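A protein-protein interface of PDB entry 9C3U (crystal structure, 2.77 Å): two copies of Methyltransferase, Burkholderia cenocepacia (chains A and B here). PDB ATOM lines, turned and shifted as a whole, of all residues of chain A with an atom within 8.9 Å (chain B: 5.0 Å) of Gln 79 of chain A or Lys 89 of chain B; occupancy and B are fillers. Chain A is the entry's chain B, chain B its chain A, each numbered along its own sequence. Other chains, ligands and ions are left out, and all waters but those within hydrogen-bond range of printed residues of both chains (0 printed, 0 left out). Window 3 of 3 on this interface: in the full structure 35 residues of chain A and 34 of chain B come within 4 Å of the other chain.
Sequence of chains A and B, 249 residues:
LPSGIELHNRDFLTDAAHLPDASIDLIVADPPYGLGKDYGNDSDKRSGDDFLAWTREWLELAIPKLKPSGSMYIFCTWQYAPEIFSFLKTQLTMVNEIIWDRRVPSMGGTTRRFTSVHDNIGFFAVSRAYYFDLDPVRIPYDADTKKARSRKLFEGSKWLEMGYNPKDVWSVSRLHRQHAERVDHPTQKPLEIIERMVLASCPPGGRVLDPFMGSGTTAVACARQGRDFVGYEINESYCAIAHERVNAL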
ATOM      1  N   TYR A  33      16.027  -0.293  11.324  1.00  0.00           N
ATOM      2  CA  TYR A  33      15.646  -0.675  12.679  1.00  0.00           C
ATOM      3  C   TYR A  33      14.595   0.246  13.282  1.00  0.00           C
ATOM      4  O   TYR A  33      13.992  -0.116  14.299  1.00  0.00           O
ATOM      5  CB  TYR A  33      16.875  -0.690  13.592  1.00  0.00           C
ATOM      6  CG  TYR A  33      17.792  -1.876  13.396  1.00  0.00           C
ATOM      7  CD1 TYR A  33      17.420  -2.945  12.592  1.00  0.00           C
ATOM      8  CD2 TYR A  33      19.025  -1.932  14.030  1.00  0.00           C
ATOM      9  CE1 TYR A  33      18.259  -4.029  12.413  1.00  0.00           C
ATOM     10  CE2 TYR A  33      19.868  -3.012  13.860  1.00  0.00           C
ATOM     11  CZ  TYR A  33      19.481  -4.058  13.052  1.00  0.00           C
ATOM     12  OH  TYR A  33      20.319  -5.136  12.882  1.00  0.00           O
ATOM     13  N   GLY A  34      14.357   1.410  12.687  1.00  0.00           N
ATOM     14  CA  GLY A  34      13.550   2.426  13.329  1.00  0.00           C
ATOM     15  C   GLY A  34      14.367   3.136  14.387  1.00  0.00           C
ATOM     16  O   GLY A  34      13.985   3.176  15.561  1.00  0.00           O
ATOM     17  N   LEU A  35      15.503   3.701  13.975  1.00  0.00           N
ATOM     18  CA  LEU A  35      16.474   4.255  14.906  1.00  0.00           C
ATOM     19  C   LEU A  35      16.949   5.656  14.543  1.00  0.00           C
ATOM     20  O   LEU A  35      17.765   6.221  15.279  1.00  0.00           O
ATOM     21  CB  LEU A  35      17.689   3.323  15.006  1.00  0.00           C
ATOM     22  CG  LEU A  35      17.663   2.293  16.133  1.00  0.00           C
ATOM     23  CD1 LEU A  35      19.063   1.777  16.376  1.00  0.00           C
ATOM     24  CD2 LEU A  35      17.077   2.886  17.409  1.00  0.00           C
ATOM     25  N   GLY A  36      16.478   6.228  13.438  1.00  0.00           N
ATOM     26  CA  GLY A  36      16.856   7.576  13.066  1.00  0.00           C
ATOM     27  C   GLY A  36      18.115   7.699  12.239  1.00  0.00           C
ATOM     28  O   GLY A  36      18.667   8.801  12.142  1.00  0.00           O
ATOM     29  N   SER A  47       8.946   5.487  13.544  1.00  0.00           N
ATOM     30  CA  SER A  47       9.019   4.925  14.884  1.00  0.00           C
ATOM     31  C   SER A  47       7.625   4.505  15.322  1.00  0.00           C
ATOM     32  O   SER A  47       6.617   4.898  14.728  1.00  0.00           O
ATOM     33  CB  SER A  47       9.624   5.920  15.882  1.00  0.00           C
ATOM     34  OG  SER A  47      10.932   6.306  15.498  1.00  0.00           O
ATOM     35  N   GLY A  48       7.584   3.688  16.372  1.00  0.00           N
ATOM     36  CA  GLY A  48       6.319   3.270  16.950  1.00  0.00           C
ATOM     37  C   GLY A  48       5.440   2.533  15.960  1.00  0.00           C
ATOM     38  O   GLY A  48       5.900   1.700  15.163  1.00  0.00           O
ATOM     39  N   PHE A  51       6.408   2.751  12.223  1.00  0.00           N
ATOM     40  CA  PHE A  51       7.440   1.793  11.849  1.00  0.00           C
ATOM     41  C   PHE A  51       6.889   0.376  11.778  1.00  0.00           C
ATOM     42  O   PHE A  51       7.223  -0.379  10.861  1.00  0.00           O
ATOM     43  CB  PHE A  51       8.600   1.856  12.840  1.00  0.00           C
ATOM     44  CG  PHE A  51       9.667   0.842  12.571  1.00  0.00           C
ATOM     45  CD1 PHE A  51      10.254   0.760  11.320  1.00  0.00           C
ATOM     46  CD2 PHE A  51      10.075  -0.039  13.558  1.00  0.00           C
ATOM     47  CE1 PHE A  51      11.229  -0.175  11.061  1.00  0.00           C
ATOM     48  CE2 PHE A  51      11.053  -0.978  13.305  1.00  0.00           C
ATOM     49  CZ  PHE A  51      11.630  -1.046  12.057  1.00  0.00           C
ATOM     50  N   LEU A  52       6.035   0.000  12.732  1.00  0.00           N
ATOM     51  CA  LEU A  52       5.589  -1.390  12.792  1.00  0.00           C
ATOM     52  C   LEU A  52       4.596  -1.719  11.682  1.00  0.00           C
ATOM     53  O   LEU A  52       4.632  -2.819  11.116  1.00  0.00           O
ATOM     54  CB  LEU A  52       4.989  -1.676  14.162  1.00  0.00           C
ATOM     55  CG  LEU A  52       6.069  -2.046  15.172  1.00  0.00           C
ATOM     56  CD1 LEU A  52       5.436  -2.548  16.439  1.00  0.00           C
ATOM     57  CD2 LEU A  52       7.005  -3.086  14.572  1.00  0.00           C
ATOM     58  N   CYS A  76      16.687  -6.756  13.447  1.00  0.00           N
ATOM     59  CA  CYS A  76      15.884  -5.754  14.133  1.00  0.00           C
ATOM     60  C   CYS A  76      16.557  -5.401  15.453  1.00  0.00           C
ATOM     61  O   CYS A  76      17.556  -6.009  15.858  1.00  0.00           O
ATOM     62  CB  CYS A  76      14.446  -6.234  14.358  1.00  0.00           C
ATOM     63  SG  CYS A  76      14.293  -7.754  15.320  1.00  0.00           S
ATOM     64  N   THR A  77      15.997  -4.391  16.109  1.00  0.00           N
ATOM     65  CA  THR A  77      16.426  -3.951  17.425  1.00  0.00           C
ATOM     66  C   THR A  77      15.495  -4.512  18.490  1.00  0.00           C
ATOM     67  O   THR A  77      14.343  -4.863  18.223  1.00  0.00           O
ATOM     68  CB  THR A  77      16.451  -2.421  17.511  1.00  0.00           C
ATOM     69  OG1 THR A  77      16.544  -2.021  18.884  1.00  0.00           O
ATOM     70  CG2 THR A  77      15.185  -1.835  16.905  1.00  0.00           C
ATOM     71  N   TRP A  78      16.017  -4.595  19.714  1.00  0.00           N
ATOM     72  CA  TRP A  78      15.227  -5.094  20.832  1.00  0.00           C
ATOM     73  C   TRP A  78      14.018  -4.214  21.124  1.00  0.00           C
ATOM     74  O   TRP A  78      13.038  -4.699  21.701  1.00  0.00           O
ATOM     75  CB  TRP A  78      16.110  -5.198  22.074  1.00  0.00           C
ATOM     76  CG  TRP A  78      16.679  -3.883  22.486  1.00  0.00           C
ATOM     77  CD1 TRP A  78      17.828  -3.305  22.029  1.00  0.00           C
ATOM     78  CD2 TRP A  78      16.118  -2.968  23.433  1.00  0.00           C
ATOM     79  NE1 TRP A  78      18.020  -2.088  22.638  1.00  0.00           N
ATOM     80  CE2 TRP A  78      16.984  -1.858  23.506  1.00  0.00           C
ATOM     81  CE3 TRP A  78      14.970  -2.982  24.229  1.00  0.00           C
ATOM     82  CZ2 TRP A  78      16.737  -0.773  24.342  1.00  0.00           C
ATOM     83  CZ3 TRP A  78      14.726  -1.904  25.060  1.00  0.00           C
ATOM     84  CH2 TRP A  78      15.605  -0.814  25.109  1.00  0.00           C
ATOM     85  N   GLN A  79      14.036  -2.964  20.684  1.00  0.00           N
ATOM     86  CA  GLN A  79      12.928  -2.033  20.993  1.00  0.00           C
ATOM     87  C   GLN A  79      11.683  -2.417  20.193  1.00  0.00           C
ATOM     88  O   GLN A  79      10.578  -2.073  20.623  1.00  0.00           O
ATOM     89  CB  GLN A  79      13.385  -0.621  20.649  1.00  0.00           C
ATOM     90  CG  GLN A  79      14.780  -0.280  21.157  1.00  0.00           C
ATOM     91  CD  GLN A  79      14.990   1.205  21.348  1.00  0.00           C
ATOM     92  OE1 GLN A  79      15.426   1.915  20.438  1.00  0.00           O
ATOM     93  NE2 GLN A  79      14.675   1.688  22.538  1.00  0.00           N
ATOM     94  N   TYR A  80      11.867  -3.088  19.066  1.00  0.00           N
ATOM     95  CA  TYR A  80      10.739  -3.497  18.245  1.00  0.00           C
ATOM     96  C   TYR A  80      10.707  -4.994  17.969  1.00  0.00           C
ATOM     97  O   TYR A  80       9.771  -5.462  17.313  1.00  0.00           O
ATOM     98  CB  TYR A  80      10.746  -2.740  16.909  1.00  0.00           C
ATOM     99  CG  TYR A  80      10.598  -1.245  17.055  1.00  0.00           C
ATOM    100  CD1 TYR A  80       9.375  -0.679  17.388  1.00  0.00           C
ATOM    101  CD2 TYR A  80      11.681  -0.399  16.859  1.00  0.00           C
ATOM    102  CE1 TYR A  80       9.235   0.687  17.521  1.00  0.00           C
ATOM    103  CE2 TYR A  80      11.551   0.969  16.990  1.00  0.00           C
ATOM    104  CZ  TYR A  80      10.326   1.507  17.322  1.00  0.00           C
ATOM    105  OH  TYR A  80      10.190   2.869  17.455  1.00  0.00           O
ATOM    106  N   ALA A  81      11.696  -5.751  18.448  1.00  0.00           N
ATOM    107  CA  ALA A  81      11.726  -7.191  18.195  1.00  0.00           C
ATOM    108  C   ALA A  81      10.514  -7.926  18.754  1.00  0.00           C
ATOM    109  O   ALA A  81       9.965  -8.783  18.039  1.00  0.00           O
ATOM    110  CB  ALA A  81      13.030  -7.784  18.737  1.00  0.00           C
ATOM    111  N   PRO A  82      10.060  -7.682  19.993  1.00  0.00           N
ATOM    112  CA  PRO A  82       8.860  -8.395  20.470  1.00  0.00           C
ATOM    113  C   PRO A  82       7.683  -8.299  19.513  1.00  0.00           C
ATOM    114  O   PRO A  82       7.091  -9.325  19.159  1.00  0.00           O
ATOM    115  CB  PRO A  82       8.570  -7.720  21.823  1.00  0.00           C
ATOM    116  CG  PRO A  82       9.427  -6.486  21.854  1.00  0.00           C
ATOM    117  CD  PRO A  82      10.631  -6.848  21.064  1.00  0.00           C
ATOM    118  N   GLU A  83       7.367  -7.097  19.036  1.00  0.00           N
ATOM    119  CA  GLU A  83       6.204  -6.917  18.173  1.00  0.00           C
ATOM    120  C   GLU A  83       6.411  -7.560  16.805  1.00  0.00           C
ATOM    121  O   GLU A  83       5.518  -8.244  16.288  1.00  0.00           O
ATOM    122  CB  GLU A  83       5.903  -5.432  18.021  1.00  0.00           C
ATOM    123  CG  GLU A  83       5.072  -4.838  19.138  1.00  0.00           C
ATOM    124  CD  GLU A  83       5.889  -4.554  20.378  1.00  0.00           C
ATOM    125  OE1 GLU A  83       7.131  -4.461  20.267  1.00  0.00           O
ATOM    126  OE2 GLU A  83       5.284  -4.426  21.464  1.00  0.00           O
ATOM    127  N   ILE A  84       7.573  -7.327  16.190  1.00  0.00           N
ATOM    128  CA  ILE A  84       7.837  -7.867  14.858  1.00  0.00           C
ATOM    129  C   ILE A  84       7.799  -9.391  14.888  1.00  0.00           C
ATOM    130  O   ILE A  84       7.158 -10.036  14.046  1.00  0.00           O
ATOM    131  CB  ILE A  84       9.185  -7.343  14.328  1.00  0.00           C
ATOM    132  CG1 ILE A  84       9.071  -5.870  13.931  1.00  0.00           C
ATOM    133  CG2 ILE A  84       9.659  -8.165  13.146  1.00  0.00           C
ATOM    134  CD1 ILE A  84      10.397  -5.142  13.903  1.00  0.00           C
ATOM    135  N   SER A 116      24.258  -1.043  24.293  1.00  0.00           N
ATOM    136  CA  SER A 116      23.841  -2.095  23.330  1.00  0.00           C
ATOM    137  C   SER A 116      25.036  -2.694  22.587  1.00  0.00           C
ATOM    138  O   SER A 116      25.885  -1.912  22.155  1.00  0.00           O
ATOM    139  CB  SER A 116      22.843  -1.554  22.349  1.00  0.00           C
ATOM    140  OG  SER A 116      22.430  -2.567  21.443  1.00  0.00           O
ATOM    141  N   HIS A 118      24.136  -5.824  20.926  1.00  0.00           N
ATOM    142  CA  HIS A 118      23.412  -6.993  20.375  1.00  0.00           C
ATOM    143  C   HIS A 118      22.380  -6.546  19.353  1.00  0.00           C
ATOM    144  O   HIS A 118      21.720  -5.515  19.552  1.00  0.00           O
ATOM    145  CB  HIS A 118      22.782  -7.845  21.486  1.00  0.00           C
ATOM    146  CG  HIS A 118      21.360  -7.563  21.819  1.00  0.00           C
ATOM    147  ND1 HIS A 118      20.996  -6.786  22.894  1.00  0.00           N
ATOM    148  CD2 HIS A 118      20.221  -7.967  21.254  1.00  0.00           C
ATOM    149  CE1 HIS A 118      19.677  -6.711  22.950  1.00  0.00           C
ATOM    150  NE2 HIS A 118      19.186  -7.423  21.962  1.00  0.00           N
ATOM    151  N   ASP A 119      22.275  -7.302  18.267  1.00  0.00           N
ATOM    152  CA  ASP A 119      21.184  -7.033  17.299  1.00  0.00           C
ATOM    153  C   ASP A 119      20.387  -8.330  17.199  1.00  0.00           C
ATOM    154  O   ASP A 119      21.004  -9.400  17.251  1.00  0.00           O
ATOM    155  CB  ASP A 119      21.722  -6.545  15.967  1.00  0.00           C
ATOM    156  CG  ASP A 119      22.092  -5.075  15.872  1.00  0.00           C
ATOM    157  OD1 ASP A 119      21.847  -4.342  16.843  1.00  0.00           O
ATOM    158  OD2 ASP A 119      22.620  -4.678  14.817  1.00  0.00           O
ATOM    159  N   ASN A 120      19.070  -8.246  17.080  1.00  0.00           N
ATOM    160  CA  ASN A 120      18.236  -9.438  17.073  1.00  0.00           C
ATOM    161  C   ASN A 120      17.989  -9.884  15.640  1.00  0.00           C
ATOM    162  O   ASN A 120      17.797  -9.056  14.747  1.00  0.00           O
ATOM    163  CB  ASN A 120      16.906  -9.176  17.784  1.00  0.00           C
ATOM    164  CG  ASN A 120      17.089  -8.817  19.245  1.00  0.00           C
ATOM    165  OD1 ASN A 120      17.567  -7.730  19.574  1.00  0.00           O
ATOM    166  ND2 ASN A 120      16.712  -9.732  20.132  1.00  0.00           N
ATOM    167  N   PHE B  85       7.168 -10.011  26.277  1.00  0.00           N
ATOM    168  CA  PHE B  85       7.686  -8.648  26.236  1.00  0.00           C
ATOM    169  C   PHE B  85       6.674  -7.689  25.619  1.00  0.00           C
ATOM    170  O   PHE B  85       6.519  -6.557  26.092  1.00  0.00           O
ATOM    171  CB  PHE B  85       9.003  -8.610  25.459  1.00  0.00           C
ATOM    172  CG  PHE B  85      10.154  -9.262  26.176  1.00  0.00           C
ATOM    173  CD1 PHE B  85      10.055  -9.605  27.515  1.00  0.00           C
ATOM    174  CD2 PHE B  85      11.334  -9.536  25.504  1.00  0.00           C
ATOM    175  CE1 PHE B  85      11.114 -10.207  28.169  1.00  0.00           C
ATOM    176  CE2 PHE B  85      12.395 -10.137  26.152  1.00  0.00           C
ATOM    177  CZ  PHE B  85      12.285 -10.472  27.487  1.00  0.00           C
ATOM    178  N   SER B  86       5.980  -8.120  24.560  1.00  0.00           N
ATOM    179  CA  SER B  86       4.958  -7.282  23.947  1.00  0.00           C
ATOM    180  C   SER B  86       3.829  -6.987  24.919  1.00  0.00           C
ATOM    181  O   SER B  86       3.247  -5.897  24.885  1.00  0.00           O
ATOM    182  CB  SER B  86       4.416  -7.963  22.689  1.00  0.00           C
ATOM    183  OG  SER B  86       3.757  -7.039  21.841  1.00  0.00           O
ATOM    184  N   PHE B  87       3.503  -7.940  25.792  1.00  0.00           N
ATOM    185  CA  PHE B  87       2.495  -7.667  26.809  1.00  0.00           C
ATOM    186  C   PHE B  87       3.026  -6.711  27.870  1.00  0.00           C
ATOM    187  O   PHE B  87       2.326  -5.780  28.282  1.00  0.00           O
ATOM    188  CB  PHE B  87       2.019  -8.958  27.470  1.00  0.00           C
ATOM    189  CG  PHE B  87       1.420  -8.741  28.828  1.00  0.00           C
ATOM    190  CD1 PHE B  87       0.173  -8.150  28.960  1.00  0.00           C
ATOM    191  CD2 PHE B  87       2.112  -9.096  29.974  1.00  0.00           C
ATOM    192  CE1 PHE B  87      -0.378  -7.934  30.208  1.00  0.00           C
ATOM    193  CE2 PHE B  87       1.567  -8.880  31.225  1.00  0.00           C
ATOM    194  CZ  PHE B  87       0.319  -8.297  31.343  1.00  0.00           C
ATOM    195  N   LEU B  88       4.259  -6.934  28.334  1.00  0.00           N
ATOM    196  CA  LEU B  88       4.798  -6.104  29.406  1.00  0.00           C
ATOM    197  C   LEU B  88       5.036  -4.671  28.951  1.00  0.00           C
ATOM    198  O   LEU B  88       5.034  -3.751  29.777  1.00  0.00           O
ATOM    199  CB  LEU B  88       6.092  -6.712  29.948  1.00  0.00           C
ATOM    200  CG  LEU B  88       5.993  -8.102  30.576  1.00  0.00           C
ATOM    201  CD1 LEU B  88       7.322  -8.540  31.161  1.00  0.00           C
ATOM    202  CD2 LEU B  88       4.943  -8.077  31.659  1.00  0.00           C
ATOM    203  N   LYS B  89       5.240  -4.458  27.650  1.00  0.00           N
ATOM    204  CA  LYS B  89       5.418  -3.101  27.153  1.00  0.00           C
ATOM    205  C   LYS B  89       4.149  -2.269  27.280  1.00  0.00           C
ATOM    206  O   LYS B  89       4.229  -1.036  27.302  1.00  0.00           O
ATOM    207  CB  LYS B  89       5.888  -3.129  25.699  1.00  0.00           C
ATOM    208  CG  LYS B  89       7.320  -3.613  25.535  1.00  0.00           C
ATOM    209  CD  LYS B  89       8.074  -2.802  24.494  1.00  0.00           C
ATOM    210  CE  LYS B  89       7.558  -3.105  23.101  1.00  0.00           C
ATOM    211  NZ  LYS B  89       8.458  -2.607  22.027  1.00  0.00           N
ATOM    212  N   THR B  90       2.983  -2.914  27.369  1.00  0.00           N
ATOM    213  CA  THR B  90       1.741  -2.185  27.587  1.00  0.00           C
ATOM    214  C   THR B  90       1.597  -1.729  29.032  1.00  0.00           C
ATOM    215  O   THR B  90       0.945  -0.713  29.297  1.00  0.00           O
ATOM    216  CB  THR B  90       0.544  -3.054  27.201  1.00  0.00           C
ATOM    217  OG1 THR B  90       0.407  -4.127  28.143  1.00  0.00           O
ATOM    218  CG2 THR B  90       0.735  -3.632  25.807  1.00  0.00           C
ATOM    219  N   GLN B  91       2.196  -2.458  29.973  1.00  0.00           N
ATOM    220  CA  GLN B  91       2.089  -2.130  31.388  1.00  0.00           C
ATOM    221  C   GLN B  91       3.237  -1.252  31.869  1.00  0.00           C
ATOM    222  O   GLN B  91       3.015  -0.312  32.641  1.00  0.00           O
ATOM    223  CB  GLN B  91       2.032  -3.414  32.219  1.00  0.00           C
ATOM    224  CG  GLN B  91       1.288  -4.553  31.541  1.00  0.00           C
ATOM    225  CD  GLN B  91      -0.142  -4.687  32.025  1.00  0.00           C
ATOM    226  OE1 GLN B  91      -0.420  -4.551  33.217  1.00  0.00           O
ATOM    227  NE2 GLN B  91      -1.059  -4.945  31.100  1.00  0.00           N
ATOM    228  N   LEU B  92       4.462  -1.542  31.434  1.00  0.00           N
ATOM    229  CA  LEU B  92       5.652  -0.812  31.847  1.00  0.00           C
ATOM    230  C   LEU B  92       6.462  -0.441  30.610  1.00  0.00           C
ATOM    231  O   LEU B  92       6.115  -0.799  29.481  1.00  0.00           O
ATOM    232  CB  LEU B  92       6.500  -1.641  32.823  1.00  0.00           C
ATOM    233  CG  LEU B  92       5.811  -2.629  33.772  1.00  0.00           C
ATOM    234  CD1 LEU B  92       6.848  -3.427  34.545  1.00  0.00           C
ATOM    235  CD2 LEU B  92       4.882  -1.913  34.741  1.00  0.00           C
ATOM    236  N   MET B  94      10.132  -0.684  28.606  1.00  0.00           N
ATOM    237  CA  MET B  94      11.294  -1.555  28.491  1.00  0.00           C
ATOM    238  C   MET B  94      12.561  -0.711  28.468  1.00  0.00           C
ATOM    239  O   MET B  94      12.779   0.068  27.534  1.00  0.00           O
ATOM    240  CB  MET B  94      11.216  -2.425  27.238  1.00  0.00           C
ATOM    241  CG  MET B  94      11.687  -3.850  27.472  1.00  0.00           C
ATOM    242  SD  MET B  94      11.630  -4.897  26.008  1.00  0.00           S
ATOM    243  CE  MET B  94      12.974  -6.026  26.369  1.00  0.00           C
ATOM    244  N   PHE B 124      12.514  -3.968  32.542  1.00  0.00           N
ATOM    245  CA  PHE B 124      11.414  -3.023  32.479  1.00  0.00           C
ATOM    246  C   PHE B 124      11.464  -2.092  33.682  1.00  0.00           C
ATOM    247  O   PHE B 124      12.128  -2.372  34.684  1.00  0.00           O
ATOM    248  CB  PHE B 124      10.062  -3.749  32.454  1.00  0.00           C
ATOM    249  CG  PHE B 124       9.896  -4.687  31.293  1.00  0.00           C
ATOM    250  CD1 PHE B 124      10.410  -5.971  31.346  1.00  0.00           C
ATOM    251  CD2 PHE B 124       9.206  -4.292  30.158  1.00  0.00           C
ATOM    252  CE1 PHE B 124      10.257  -6.839  30.283  1.00  0.00           C
ATOM    253  CE2 PHE B 124       9.044  -5.160  29.093  1.00  0.00           C
ATOM    254  CZ  PHE B 124       9.573  -6.434  29.156  1.00  0.00           C
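Gln 79 of chain A touches just one residue of chain B: Lys 89 (2.6 Å). Of the printed residues of chain A, Lys 89 of chain B touches Gln 79 and Glu 83. No residue of chain A comes within 4 Å of Thr 90 of chain B. Of the printed residues of chain A, Met 94 of chain B touches Trp 78 (3.7 Å). Printed residues of chain B within 4 Å of Pro 82 of chain A: Phe 85 (3.8 Å) and Ser 86 (3.8 Å). Of the printed residues of chain B, Trp 78 of chain A touches Met 94 (3.7 Å). Printed residues of chain A within 4 Å of Ser 86 of chain B: Pro 82 (3.8 Å) and Glu 83 (3.0 Å). Printed residues of chain B within 4 Å of Glu 83 of chain A: Ser 86 and Lys 89. Thr 77 of chain A touches none of the printed residues of chain B. Ala 81 of chain A touches none of the printed residues of chain B.
The side-chain hydroxyl (OG) of Ser 86 of chain B lies within hydrogen-bond range of the side-chain carboxylate (OE2) of Glu 83 of chain A. The side-chain amino group (NZ) of Lys 89 of chain B is in hydrogen-bond range of the backbone carbonyl oxygen (O) of Gln 79 of chain A, 2.6 Å away. The side-chain carboxylate (OE1) of Glu 83 of chain A is in salt-bridge range of the side-chain amino group (NZ) of Lys 89 of chain B (2.9 Å).
Printed residues of chain B that touch a printed residue of chain A: Phe 85, Ser 86, Lys 89 and Met 94. Hydrophobic or aromatic side chains of chain B within 4 Å of the printed part of chain A: Phe 85. Hydrophobic or aromatic side chains of chain A that line the printed part of chain B: Trp 78 and Pro 82. Among the printed residues, 6 pairs touch across the chains.
Among the printed residues, merely in contact across the chains: Trp 78 of chain A with Met 94 of chain B (3.7 Å), Pro 82 of chain A with Phe 85 of chain B (3.8 Å) and Pro 82 of chain A with Ser 86 of chain B (3.8 Å).
N of Gln 79 of chain A sits close to OG1 of Thr 77 of chain A, 3.2 Å away. N of Trp 78 of chain A lies close to OD1 of Asn 120 of chain A (3.5 Å).
No position is printed for both chains.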
